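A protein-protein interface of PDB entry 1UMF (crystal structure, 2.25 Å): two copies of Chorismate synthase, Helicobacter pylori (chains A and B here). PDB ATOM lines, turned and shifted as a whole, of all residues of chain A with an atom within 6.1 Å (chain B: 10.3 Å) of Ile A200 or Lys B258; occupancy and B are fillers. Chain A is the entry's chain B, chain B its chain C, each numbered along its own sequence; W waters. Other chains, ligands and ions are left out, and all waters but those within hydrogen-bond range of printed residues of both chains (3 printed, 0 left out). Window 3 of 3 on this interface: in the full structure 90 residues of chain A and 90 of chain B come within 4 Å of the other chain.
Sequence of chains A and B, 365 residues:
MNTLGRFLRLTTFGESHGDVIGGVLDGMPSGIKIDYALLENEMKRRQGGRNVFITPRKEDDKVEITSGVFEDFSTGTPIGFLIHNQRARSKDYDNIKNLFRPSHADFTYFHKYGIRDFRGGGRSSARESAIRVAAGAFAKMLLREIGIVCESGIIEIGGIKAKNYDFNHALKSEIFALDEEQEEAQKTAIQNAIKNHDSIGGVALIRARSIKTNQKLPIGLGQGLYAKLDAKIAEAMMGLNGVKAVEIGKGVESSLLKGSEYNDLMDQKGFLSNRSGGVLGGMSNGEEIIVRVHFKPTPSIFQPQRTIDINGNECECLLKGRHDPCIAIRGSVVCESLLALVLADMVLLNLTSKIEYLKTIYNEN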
ATOM      1  N   ILE A 157       3.412  13.094   5.362  1.00  0.00           N
ATOM      2  CA  ILE A 157       4.527  13.583   4.568  1.00  0.00           C
ATOM      3  C   ILE A 157       5.771  13.588   5.444  1.00  0.00           C
ATOM      4  O   ILE A 157       5.789  14.203   6.509  1.00  0.00           O
ATOM      5  CB  ILE A 157       4.290  15.011   4.061  1.00  0.00           C
ATOM      6  CG1 ILE A 157       3.117  15.022   3.074  1.00  0.00           C
ATOM      7  CG2 ILE A 157       5.572  15.540   3.423  1.00  0.00           C
ATOM      8  CD1 ILE A 157       2.915  16.341   2.341  1.00  0.00           C
ATOM      9  N   GLY A 158       6.813  12.904   4.998  1.00  0.00           N
ATOM     10  CA  GLY A 158       8.026  12.860   5.784  1.00  0.00           C
ATOM     11  C   GLY A 158       7.767  12.337   7.182  1.00  0.00           C
ATOM     12  O   GLY A 158       8.417  12.759   8.134  1.00  0.00           O
ATOM     13  N   GLN A 186       3.882  19.744   7.619  1.00  0.00           N
ATOM     14  CA  GLN A 186       4.053  18.933   6.422  1.00  0.00           C
ATOM     15  C   GLN A 186       4.646  19.763   5.287  1.00  0.00           C
ATOM     16  O   GLN A 186       5.534  19.295   4.577  1.00  0.00           O
ATOM     17  CB  GLN A 186       2.709  18.327   6.008  1.00  0.00           C
ATOM     18  CG  GLN A 186       2.299  17.135   6.863  1.00  0.00           C
ATOM     19  CD  GLN A 186       0.849  16.729   6.665  1.00  0.00           C
ATOM     20  OE1 GLN A 186       0.438  15.639   7.075  1.00  0.00           O
ATOM     21  NE2 GLN A 186       0.063  17.607   6.052  1.00  0.00           N
ATOM     22  N   ALA A 189       8.255  20.495   5.825  1.00  0.00           N
ATOM     23  CA  ALA A 189       9.088  19.342   5.499  1.00  0.00           C
ATOM     24  C   ALA A 189       9.390  19.354   4.006  1.00  0.00           C
ATOM     25  O   ALA A 189      10.475  18.971   3.574  1.00  0.00           O
ATOM     26  CB  ALA A 189       8.373  18.056   5.873  1.00  0.00           C
ATOM     27  N   ILE A 190       8.417  19.793   3.218  1.00  0.00           N
ATOM     28  CA  ILE A 190       8.595  19.859   1.777  1.00  0.00           C
ATOM     29  C   ILE A 190       9.601  20.948   1.418  1.00  0.00           C
ATOM     30  O   ILE A 190      10.416  20.769   0.517  1.00  0.00           O
ATOM     31  CB  ILE A 190       7.256  20.140   1.057  1.00  0.00           C
ATOM     32  CG1 ILE A 190       6.319  18.942   1.229  1.00  0.00           C
ATOM     33  CG2 ILE A 190       7.504  20.404  -0.420  1.00  0.00           C
ATOM     34  CD1 ILE A 190       4.999  19.084   0.510  1.00  0.00           C
ATOM     35  N   ALA A 193      13.127  19.770   2.037  1.00  0.00           N
ATOM     36  CA  ALA A 193      13.562  18.800   1.038  1.00  0.00           C
ATOM     37  C   ALA A 193      14.133  19.567  -0.154  1.00  0.00           C
ATOM     38  O   ALA A 193      15.228  19.267  -0.638  1.00  0.00           O
ATOM     39  CB  ALA A 193      12.381  17.939   0.597  1.00  0.00           C
ATOM     40  N   ASP A 198      16.752  17.420  -1.798  1.00  0.00           N
ATOM     41  CA  ASP A 198      16.412  16.029  -1.525  1.00  0.00           C
ATOM     42  C   ASP A 198      14.924  15.802  -1.775  1.00  0.00           C
ATOM     43  O   ASP A 198      14.245  16.659  -2.339  1.00  0.00           O
ATOM     44  CB  ASP A 198      16.748  15.677  -0.078  1.00  0.00           C
ATOM     45  CG  ASP A 198      17.264  14.256   0.073  1.00  0.00           C
ATOM     46  OD1 ASP A 198      16.789  13.359  -0.664  1.00  0.00           O
ATOM     47  OD2 ASP A 198      18.143  14.037   0.939  1.00  0.00           O
ATOM     48  N   SER A 199      14.420  14.647  -1.351  1.00  0.00           N
ATOM     49  CA  SER A 199      13.009  14.317  -1.525  1.00  0.00           C
ATOM     50  C   SER A 199      12.487  13.519  -0.333  1.00  0.00           C
ATOM     51  O   SER A 199      13.264  12.913   0.409  1.00  0.00           O
ATOM     52  CB  SER A 199      12.807  13.514  -2.815  1.00  0.00           C
ATOM     53  OG  SER A 199      13.591  12.331  -2.802  1.00  0.00           O
ATOM     54  N   ILE A 200      11.172  13.521  -0.153  1.00  0.00           N
ATOM     55  CA  ILE A 200      10.552  12.792   0.948  1.00  0.00           C
ATOM     56  C   ILE A 200       9.365  11.951   0.493  1.00  0.00           C
ATOM     57  O   ILE A 200       8.707  12.264  -0.505  1.00  0.00           O
ATOM     58  CB  ILE A 200      10.061  13.750   2.058  1.00  0.00           C
ATOM     59  CG1 ILE A 200       9.431  14.987   1.420  1.00  0.00           C
ATOM     60  CG2 ILE A 200      11.210  14.104   2.992  1.00  0.00           C
ATOM     61  CD1 ILE A 200       8.851  15.973   2.418  1.00  0.00           C
ATOM     62  N   GLY A 201       9.101  10.884   1.238  1.00  0.00           N
ATOM     63  CA  GLY A 201       7.997  10.006   0.922  1.00  0.00           C
ATOM     64  C   GLY A 201       6.725  10.512   1.567  1.00  0.00           C
ATOM     65  O   GLY A 201       6.740  11.470   2.345  1.00  0.00           O
ATOM     66  N   GLY A 202       5.613   9.866   1.244  1.00  0.00           N
ATOM     67  CA  GLY A 202       4.344  10.268   1.808  1.00  0.00           C
ATOM     68  C   GLY A 202       3.371   9.113   1.791  1.00  0.00           C
ATOM     69  O   GLY A 202       3.659   8.047   1.249  1.00  0.00           O
ATOM     70  N   PHE A 295       4.245   5.894  -0.720  1.00  0.00           N
ATOM     71  CA  PHE A 295       5.165   6.347  -1.755  1.00  0.00           C
ATOM     72  C   PHE A 295       6.580   6.549  -1.220  1.00  0.00           C
ATOM     73  O   PHE A 295       6.775   7.159  -0.167  1.00  0.00           O
ATOM     74  CB  PHE A 295       4.706   7.680  -2.349  1.00  0.00           C
ATOM     75  CG  PHE A 295       3.465   7.590  -3.177  1.00  0.00           C
ATOM     76  CD1 PHE A 295       2.216   7.533  -2.576  1.00  0.00           C
ATOM     77  CD2 PHE A 295       3.547   7.578  -4.566  1.00  0.00           C
ATOM     78  CE1 PHE A 295       1.056   7.468  -3.350  1.00  0.00           C
ATOM     79  CE2 PHE A 295       2.401   7.514  -5.345  1.00  0.00           C
ATOM     80  CZ  PHE A 295       1.151   7.460  -4.739  1.00  0.00           C
ATOM     81  N   LYS A 296       7.563   6.038  -1.948  1.00  0.00           N
ATOM     82  CA  LYS A 296       8.962   6.219  -1.579  1.00  0.00           C
ATOM     83  C   LYS A 296       9.273   7.663  -1.990  1.00  0.00           C
ATOM     84  O   LYS A 296       8.514   8.274  -2.748  1.00  0.00           O
ATOM     85  CB  LYS A 296       9.853   5.276  -2.393  1.00  0.00           C
ATOM     86  CG  LYS A 296       9.753   5.522  -3.895  1.00  0.00           C
ATOM     87  CD  LYS A 296      10.788   4.741  -4.697  1.00  0.00           C
ATOM     88  CE  LYS A 296      10.674   5.076  -6.179  1.00  0.00           C
ATOM     89  NZ  LYS A 296      11.655   4.344  -7.032  1.00  0.00           N
ATOM     90  N   PRO A 297      10.380   8.234  -1.489  1.00  0.00           N
ATOM     91  CA  PRO A 297      10.713   9.612  -1.869  1.00  0.00           C
ATOM     92  C   PRO A 297      11.106   9.663  -3.347  1.00  0.00           C
ATOM     93  O   PRO A 297      11.615   8.682  -3.898  1.00  0.00           O
ATOM     94  CB  PRO A 297      11.880   9.953  -0.944  1.00  0.00           C
ATOM     95  CG  PRO A 297      12.555   8.623  -0.755  1.00  0.00           C
ATOM     96  CD  PRO A 297      11.378   7.690  -0.551  1.00  0.00           C
ATOM     97  N   THR A 298      10.864  10.802  -3.984  1.00  0.00           N
ATOM     98  CA  THR A 298      11.182  10.990  -5.396  1.00  0.00           C
ATOM     99  C   THR A 298      12.594  10.520  -5.743  1.00  0.00           C
ATOM    100  O   THR A 298      13.556  10.818  -5.032  1.00  0.00           O
ATOM    101  CB  THR A 298      11.058  12.472  -5.787  1.00  0.00           C
ATOM    102  OG1 THR A 298       9.813  12.995  -5.297  1.00  0.00           O
ATOM    103  CG2 THR A 298      11.121  12.625  -7.299  1.00  0.00           C
ATOM    104  N   PRO A 325       9.664  17.304  -4.933  1.00  0.00           N
ATOM    105  CA  PRO A 325      10.106  16.879  -3.603  1.00  0.00           C
ATOM    106  C   PRO A 325       9.303  15.724  -2.992  1.00  0.00           C
ATOM    107  O   PRO A 325       9.828  14.967  -2.177  1.00  0.00           O
ATOM    108  CB  PRO A 325       9.990  18.162  -2.782  1.00  0.00           C
ATOM    109  CG  PRO A 325       8.800  18.834  -3.402  1.00  0.00           C
ATOM    110  CD  PRO A 325       9.057  18.647  -4.886  1.00  0.00           C
ATOM    111  N   CYS A 326       8.043  15.577  -3.394  1.00  0.00           N
ATOM    112  CA  CYS A 326       7.200  14.520  -2.836  1.00  0.00           C
ATOM    113  C   CYS A 326       6.105  14.061  -3.808  1.00  0.00           C
ATOM    114  O   CYS A 326       5.018  14.645  -3.857  1.00  0.00           O
ATOM    115  CB  CYS A 326       6.570  15.031  -1.536  1.00  0.00           C
ATOM    116  SG  CYS A 326       5.599  13.839  -0.600  1.00  0.00           S
ATOM    117  N   ILE A 327       6.394  13.007  -4.568  1.00  0.00           N
ATOM    118  CA  ILE A 327       5.440  12.478  -5.546  1.00  0.00           C
ATOM    119  C   ILE A 327       4.133  11.984  -4.936  1.00  0.00           C
ATOM    120  O   ILE A 327       3.111  11.942  -5.616  1.00  0.00           O
ATOM    121  CB  ILE A 327       6.053  11.330  -6.380  1.00  0.00           C
ATOM    122  CG1 ILE A 327       6.718  10.305  -5.454  1.00  0.00           C
ATOM    123  CG2 ILE A 327       7.031  11.903  -7.410  1.00  0.00           C
ATOM    124  CD1 ILE A 327       7.280   9.090  -6.180  1.00  0.00           C
ATOM    125  N   ALA A 328       4.161  11.614  -3.660  1.00  0.00           N
ATOM    126  CA  ALA A 328       2.954  11.140  -2.988  1.00  0.00           C
ATOM    127  C   ALA A 328       1.794  12.112  -3.210  1.00  0.00           C
ATOM    128  O   ALA A 328       0.647  11.702  -3.376  1.00  0.00           O
ATOM    129  CB  ALA A 328       3.215  10.976  -1.484  1.00  0.00           C
ATOM    130  N   LYS B 250      11.560  -2.121   1.041  1.00  0.00           N
ATOM    131  CA  LYS B 250      11.438  -1.299   2.242  1.00  0.00           C
ATOM    132  C   LYS B 250       9.969  -1.098   2.660  1.00  0.00           C
ATOM    133  O   LYS B 250       9.679  -0.721   3.801  1.00  0.00           O
ATOM    134  CB  LYS B 250      12.131   0.049   2.003  1.00  0.00           C
ATOM    135  CG  LYS B 250      12.478   0.819   3.269  1.00  0.00           C
ATOM    136  CD  LYS B 250      13.457   0.039   4.146  1.00  0.00           C
ATOM    137  CE  LYS B 250      13.755   0.783   5.447  1.00  0.00           C
ATOM    138  NZ  LYS B 250      14.525  -0.040   6.426  1.00  0.00           N
ATOM    139  N   GLU B 253       8.095   1.408   5.172  1.00  0.00           N
ATOM    140  CA  GLU B 253       9.184   2.203   5.732  1.00  0.00           C
ATOM    141  C   GLU B 253       9.698   3.208   4.705  1.00  0.00           C
ATOM    142  O   GLU B 253      10.375   4.177   5.050  1.00  0.00           O
ATOM    143  CB  GLU B 253      10.330   1.295   6.182  1.00  0.00           C
ATOM    144  CG  GLU B 253      10.036   0.533   7.463  1.00  0.00           C
ATOM    145  CD  GLU B 253      11.175  -0.389   7.873  1.00  0.00           C
ATOM    146  OE1 GLU B 253      11.409  -1.403   7.179  1.00  0.00           O
ATOM    147  OE2 GLU B 253      11.841  -0.095   8.889  1.00  0.00           O
ATOM    148  N   SER B 254       9.357   2.971   3.441  1.00  0.00           N
ATOM    149  CA  SER B 254       9.784   3.838   2.350  1.00  0.00           C
ATOM    150  C   SER B 254       9.256   5.266   2.460  1.00  0.00           C
ATOM    151  O   SER B 254       9.969   6.220   2.167  1.00  0.00           O
ATOM    152  CB  SER B 254       9.345   3.246   1.009  1.00  0.00           C
ATOM    153  OG  SER B 254       9.958   1.998   0.781  1.00  0.00           O
ATOM    154  N   SER B 255       8.005   5.408   2.877  1.00  0.00           N
ATOM    155  CA  SER B 255       7.387   6.723   3.000  1.00  0.00           C
ATOM    156  C   SER B 255       8.006   7.571   4.113  1.00  0.00           C
ATOM    157  O   SER B 255       7.667   8.744   4.266  1.00  0.00           O
ATOM    158  CB  SER B 255       5.886   6.560   3.237  1.00  0.00           C
ATOM    159  OG  SER B 255       5.649   5.612   4.267  1.00  0.00           O
ATOM    160  N   LEU B 256       8.915   6.979   4.883  1.00  0.00           N
ATOM    161  CA  LEU B 256       9.578   7.693   5.973  1.00  0.00           C
ATOM    162  C   LEU B 256      11.048   7.955   5.648  1.00  0.00           C
ATOM    163  O   LEU B 256      11.813   8.399   6.503  1.00  0.00           O
ATOM    164  CB  LEU B 256       9.489   6.889   7.274  1.00  0.00           C
ATOM    165  CG  LEU B 256       8.090   6.467   7.732  1.00  0.00           C
ATOM    166  CD1 LEU B 256       8.201   5.674   9.022  1.00  0.00           C
ATOM    167  CD2 LEU B 256       7.215   7.692   7.930  1.00  0.00           C
ATOM    168  N   LEU B 257      11.444   7.671   4.417  1.00  0.00           N
ATOM    169  CA  LEU B 257      12.824   7.884   4.015  1.00  0.00           C
ATOM    170  C   LEU B 257      12.962   9.068   3.068  1.00  0.00           C
ATOM    171  O   LEU B 257      11.983   9.529   2.476  1.00  0.00           O
ATOM    172  CB  LEU B 257      13.372   6.627   3.333  1.00  0.00           C
ATOM    173  CG  LEU B 257      14.133   5.572   4.145  1.00  0.00           C
ATOM    174  CD1 LEU B 257      13.409   5.225   5.429  1.00  0.00           C
ATOM    175  CD2 LEU B 257      14.310   4.340   3.279  1.00  0.00           C
ATOM    176  N   LYS B 258      14.187   9.564   2.942  1.00  0.00           N
ATOM    177  CA  LYS B 258      14.474  10.665   2.040  1.00  0.00           C
ATOM    178  C   LYS B 258      15.177  10.052   0.841  1.00  0.00           C
ATOM    179  O   LYS B 258      15.841   9.021   0.965  1.00  0.00           O
ATOM    180  CB  LYS B 258      15.392  11.693   2.702  1.00  0.00           C
ATOM    181  CG  LYS B 258      14.736  12.505   3.798  1.00  0.00           C
ATOM    182  CD  LYS B 258      15.579  13.729   4.139  1.00  0.00           C
ATOM    183  CE  LYS B 258      16.872  13.358   4.844  1.00  0.00           C
ATOM    184  NZ  LYS B 258      16.614  12.909   6.244  1.00  0.00           N
ATOM    185  N   GLY B 259      15.031  10.685  -0.317  1.00  0.00           N
ATOM    186  CA  GLY B 259      15.657  10.173  -1.520  1.00  0.00           C
ATOM    187  C   GLY B 259      17.102   9.768  -1.316  1.00  0.00           C
ATOM    188  O   GLY B 259      17.502   8.671  -1.707  1.00  0.00           O
ATOM    189  N   SER B 260      17.879  10.649  -0.692  1.00  0.00           N
ATOM    190  CA  SER B 260      19.296  10.408  -0.439  1.00  0.00           C
ATOM    191  C   SER B 260      19.544   9.201   0.454  1.00  0.00           C
ATOM    192  O   SER B 260      20.669   8.708   0.546  1.00  0.00           O
ATOM    193  CB  SER B 260      19.928  11.650   0.197  1.00  0.00           C
ATOM    194  OG  SER B 260      19.284  11.987   1.412  1.00  0.00           O
ATOM    195  N   GLU B 261      18.493   8.730   1.114  1.00  0.00           N
ATOM    196  CA  GLU B 261      18.597   7.577   2.002  1.00  0.00           C
ATOM    197  C   GLU B 261      18.036   6.320   1.341  1.00  0.00           C
ATOM    198  O   GLU B 261      18.587   5.227   1.491  1.00  0.00           O
ATOM    199  CB  GLU B 261      17.825   7.843   3.296  1.00  0.00           C
ATOM    200  CG  GLU B 261      18.403   8.942   4.165  1.00  0.00           C
ATOM    201  CD  GLU B 261      17.423   9.415   5.215  1.00  0.00           C
ATOM    202  OE1 GLU B 261      17.860  10.035   6.209  1.00  0.00           O
ATOM    203  OE2 GLU B 261      16.210   9.177   5.043  1.00  0.00           O
ATOM    204  N   TYR B 262      16.938   6.493   0.611  1.00  0.00           N
ATOM    205  CA  TYR B 262      16.268   5.392  -0.071  1.00  0.00           C
ATOM    206  C   TYR B 262      16.955   4.926  -1.355  1.00  0.00           C
ATOM    207  O   TYR B 262      17.260   3.747  -1.497  1.00  0.00           O
ATOM    208  CB  TYR B 262      14.817   5.788  -0.374  1.00  0.00           C
ATOM    209  CG  TYR B 262      14.006   4.717  -1.071  1.00  0.00           C
ATOM    210  CD1 TYR B 262      14.171   4.461  -2.434  1.00  0.00           C
ATOM    211  CD2 TYR B 262      13.070   3.962  -0.367  1.00  0.00           C
ATOM    212  CE1 TYR B 262      13.422   3.483  -3.075  1.00  0.00           C
ATOM    213  CE2 TYR B 262      12.315   2.981  -0.997  1.00  0.00           C
ATOM    214  CZ  TYR B 262      12.494   2.747  -2.351  1.00  0.00           C
ATOM    215  OH  TYR B 262      11.750   1.776  -2.979  1.00  0.00           O
ATOM    216  N   ASN B 263      17.180   5.846  -2.286  1.00  0.00           N
ATOM    217  CA  ASN B 263      17.820   5.526  -3.564  1.00  0.00           C
ATOM    218  C   ASN B 263      18.940   4.488  -3.461  1.00  0.00           C
ATOM    219  O   ASN B 263      19.883   4.649  -2.679  1.00  0.00           O
ATOM    220  CB  ASN B 263      18.373   6.804  -4.201  1.00  0.00           C
ATOM    221  CG  ASN B 263      17.282   7.710  -4.724  1.00  0.00           C
ATOM    222  OD1 ASN B 263      16.148   7.673  -4.244  1.00  0.00           O
ATOM    223  ND2 ASN B 263      17.621   8.544  -5.703  1.00  0.00           N
ATOM    224  N   ASP B 264      18.831   3.424  -4.253  1.00  0.00           N
ATOM    225  CA  ASP B 264      19.843   2.373  -4.264  1.00  0.00           C
ATOM    226  C   ASP B 264      20.947   2.739  -5.248  1.00  0.00           C
ATOM    227  O   ASP B 264      20.702   2.877  -6.449  1.00  0.00           O
ATOM    228  CB  ASP B 264      19.236   1.023  -4.669  1.00  0.00           C
ATOM    229  CG  ASP B 264      18.238   0.500  -3.654  1.00  0.00           C
ATOM    230  OD1 ASP B 264      18.587   0.439  -2.455  1.00  0.00           O
ATOM    231  OD2 ASP B 264      17.107   0.141  -4.060  1.00  0.00           O
ATOM    232  N   LEU B 265      22.161   2.903  -4.732  1.00  0.00           N
ATOM    233  CA  LEU B 265      23.303   3.247  -5.567  1.00  0.00           C
ATOM    234  C   LEU B 265      23.867   1.977  -6.197  1.00  0.00           C
ATOM    235  O   LEU B 265      23.671   0.876  -5.679  1.00  0.00           O
ATOM    236  CB  LEU B 265      24.383   3.947  -4.733  1.00  0.00           C
ATOM    237  CG  LEU B 265      24.033   5.273  -4.038  1.00  0.00           C
ATOM    238  CD1 LEU B 265      23.445   6.251  -5.053  1.00  0.00           C
ATOM    239  CD2 LEU B 265      23.042   5.024  -2.907  1.00  0.00           C
ATOM    240  N   SER B 273      22.603  -1.613  -2.355  1.00  0.00           N
ATOM    241  CA  SER B 273      21.509  -1.864  -1.418  1.00  0.00           C
ATOM    242  C   SER B 273      20.266  -2.311  -2.188  1.00  0.00           C
ATOM    243  O   SER B 273      20.177  -2.111  -3.405  1.00  0.00           O
ATOM    244  CB  SER B 273      21.198  -0.604  -0.607  1.00  0.00           C
ATOM    245  OG  SER B 273      20.927   0.496  -1.455  1.00  0.00           O
ATOM    246  N   ARG B 275      16.649  -1.644  -1.290  1.00  0.00           N
ATOM    247  CA  ARG B 275      15.467  -1.103  -0.646  1.00  0.00           C
ATOM    248  C   ARG B 275      14.269  -1.256  -1.592  1.00  0.00           C
ATOM    249  O   ARG B 275      13.119  -1.211  -1.161  1.00  0.00           O
ATOM    250  CB  ARG B 275      15.706   0.367  -0.277  1.00  0.00           C
ATOM    251  CG  ARG B 275      16.974   0.565   0.563  1.00  0.00           C
ATOM    252  CD  ARG B 275      17.192   2.007   1.007  1.00  0.00           C
ATOM    253  NE  ARG B 275      18.535   2.199   1.558  1.00  0.00           N
ATOM    254  CZ  ARG B 275      19.621   2.455   0.831  1.00  0.00           C
ATOM    255  NH1 ARG B 275      19.541   2.562  -0.490  1.00  0.00           N
ATOM    256  NH2 ARG B 275      20.799   2.587   1.424  1.00  0.00           N
HETATM  257  O   HOH W   1      13.638   6.954  -4.591  1.00  0.00           O
HETATM  258  O   HOH W   2      11.943   1.210  -6.013  1.00  0.00           O
HETATM  259  O   HOH W   3       5.424   9.876   5.286  1.00  0.00           O
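Water W1 lies within hydrogen-bond range of the side-chain amide oxygen of Asn B263 and the backbone carbonyl oxygen of Pro A297. Water W3 bridges O of Ser B255 and N of Gly A158. Water W2 lies within hydrogen-bond range of the side-chain hydroxyl (OH) of Tyr B262 (3.1 Å) and the side-chain amino group (NZ) of Lys A296 (3.3 Å).
The backbone carbonyl oxygen (O) of Leu B257 sits at hydrogen-bond distance from the backbone NH (N) of Gly A201 (3.4 Å). The backbone carbonyl oxygen of Gly A201 lies close to the backbone carbonyl oxygen of Ser B255, at 3.5 Å. The backbone NH of Ser B260 is in hydrogen-bond range of the side-chain carboxylate of Asp A198 (2.9 Å). N of Gly B259 is in hydrogen-bond range of OD1 of Asp A198 (3.2 Å). The backbone carbonyl oxygen of Ser A199 lies within hydrogen-bond range of the backbone NH of Gly B259 (2.9 Å).
Among the printed residues, pairs that only touch across the chains: Asp A198 with Lys B258 (3.97 Å), Ser A199 with Lys B258 (3.0 Å), Ile A200 with Leu B257 (3.9 Å), Ile A200 with Lys B258 (3.95 Å), Gly A202 with Ser B255 (3.3 Å), Phe A295 with Ser B255 (3.3 Å), Lys A296 with Ser B254 (3.9 Å), Lys A296 with Tyr B262 (3.3 Å), Pro A297 with Ser B254 (3.4 Å), Pro A297 with Leu B257 (3.4 Å), Pro A297 with Lys B258 (3.4 Å), Pro A297 with Gly B259 (3.3 Å) and Pro A297 with Tyr B262 (3.6 Å).
Hydrophobic or aromatic side chains of chain A within 4 Å of the printed part of chain B: Ile A200 and Pro A297. Of the 16 printed residues of chain B, 7 touch a printed residue of chain A. Among the printed residues, 18 pairs touch across the chains.
No position is printed for both chains.
Gly A158 touches none of the printed residues of chain B. No residue of chain B comes within 4 Å of Ile A190. Printed residues of chain B within 4 Å of Asp A198: Lys B258 (3.97 Å), Gly B259 (3.2 Å) and Ser B260 (2.4 Å). Printed residues of chain B within 4 Å of Ser A199: Lys B258 and Gly B259. Ile A200 touches just these residues of chain B: Leu B257 and Lys B258. Printed residues of chain B within 4 Å of Lys A296: Ser B254 (3.9 Å) and Tyr B262 (3.3 Å). Cys A326 touches none of the printed residues of chain B. Printed residues of chain A within 4 Å of Leu B257: Ile A200 (3.9 Å), Gly A201 (3.4 Å) and Pro A297 (3.4 Å). Lys B258 touches just these residues of chain A: Asp A198, Ser A199, Ile A200 and Pro A297. Of the printed residues of chain A, Ser B260 touches Asp A198 (2.4 Å). The nearest residue of chain B that does not touch Ile A200 is Gly B259 (4.8 Å). The nearest printed residue of chain A that does not touch Ser B255 is Gly A158 (4.3 Å).
The side-chain amino group (NZ) of Lys B258 is in salt-bridge range of the side-chain carboxylate (OE1) of Glu B261. The guanidinium group (NH1) of Arg B275 sits at hydrogen-bond distance from the backbone carbonyl oxygen (O) of Tyr B262 (2.8 Å). The backbone carbonyl oxygen (O) of Ala A193 lies within hydrogen-bond range of the backbone NH (N) of Asp A198 (2.7 Å). O of Pro A325 is in hydrogen-bond range of N of Ile A200. The backbone carbonyl oxygen (O) of Gly A201 is in hydrogen-bond range of the backbone NH (N) of Gly A158 (3.0 Å). The backbone carbonyl oxygen of Gly A202 lies within hydrogen-bond range of the backbone NH of Phe A295 (3.0 Å).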
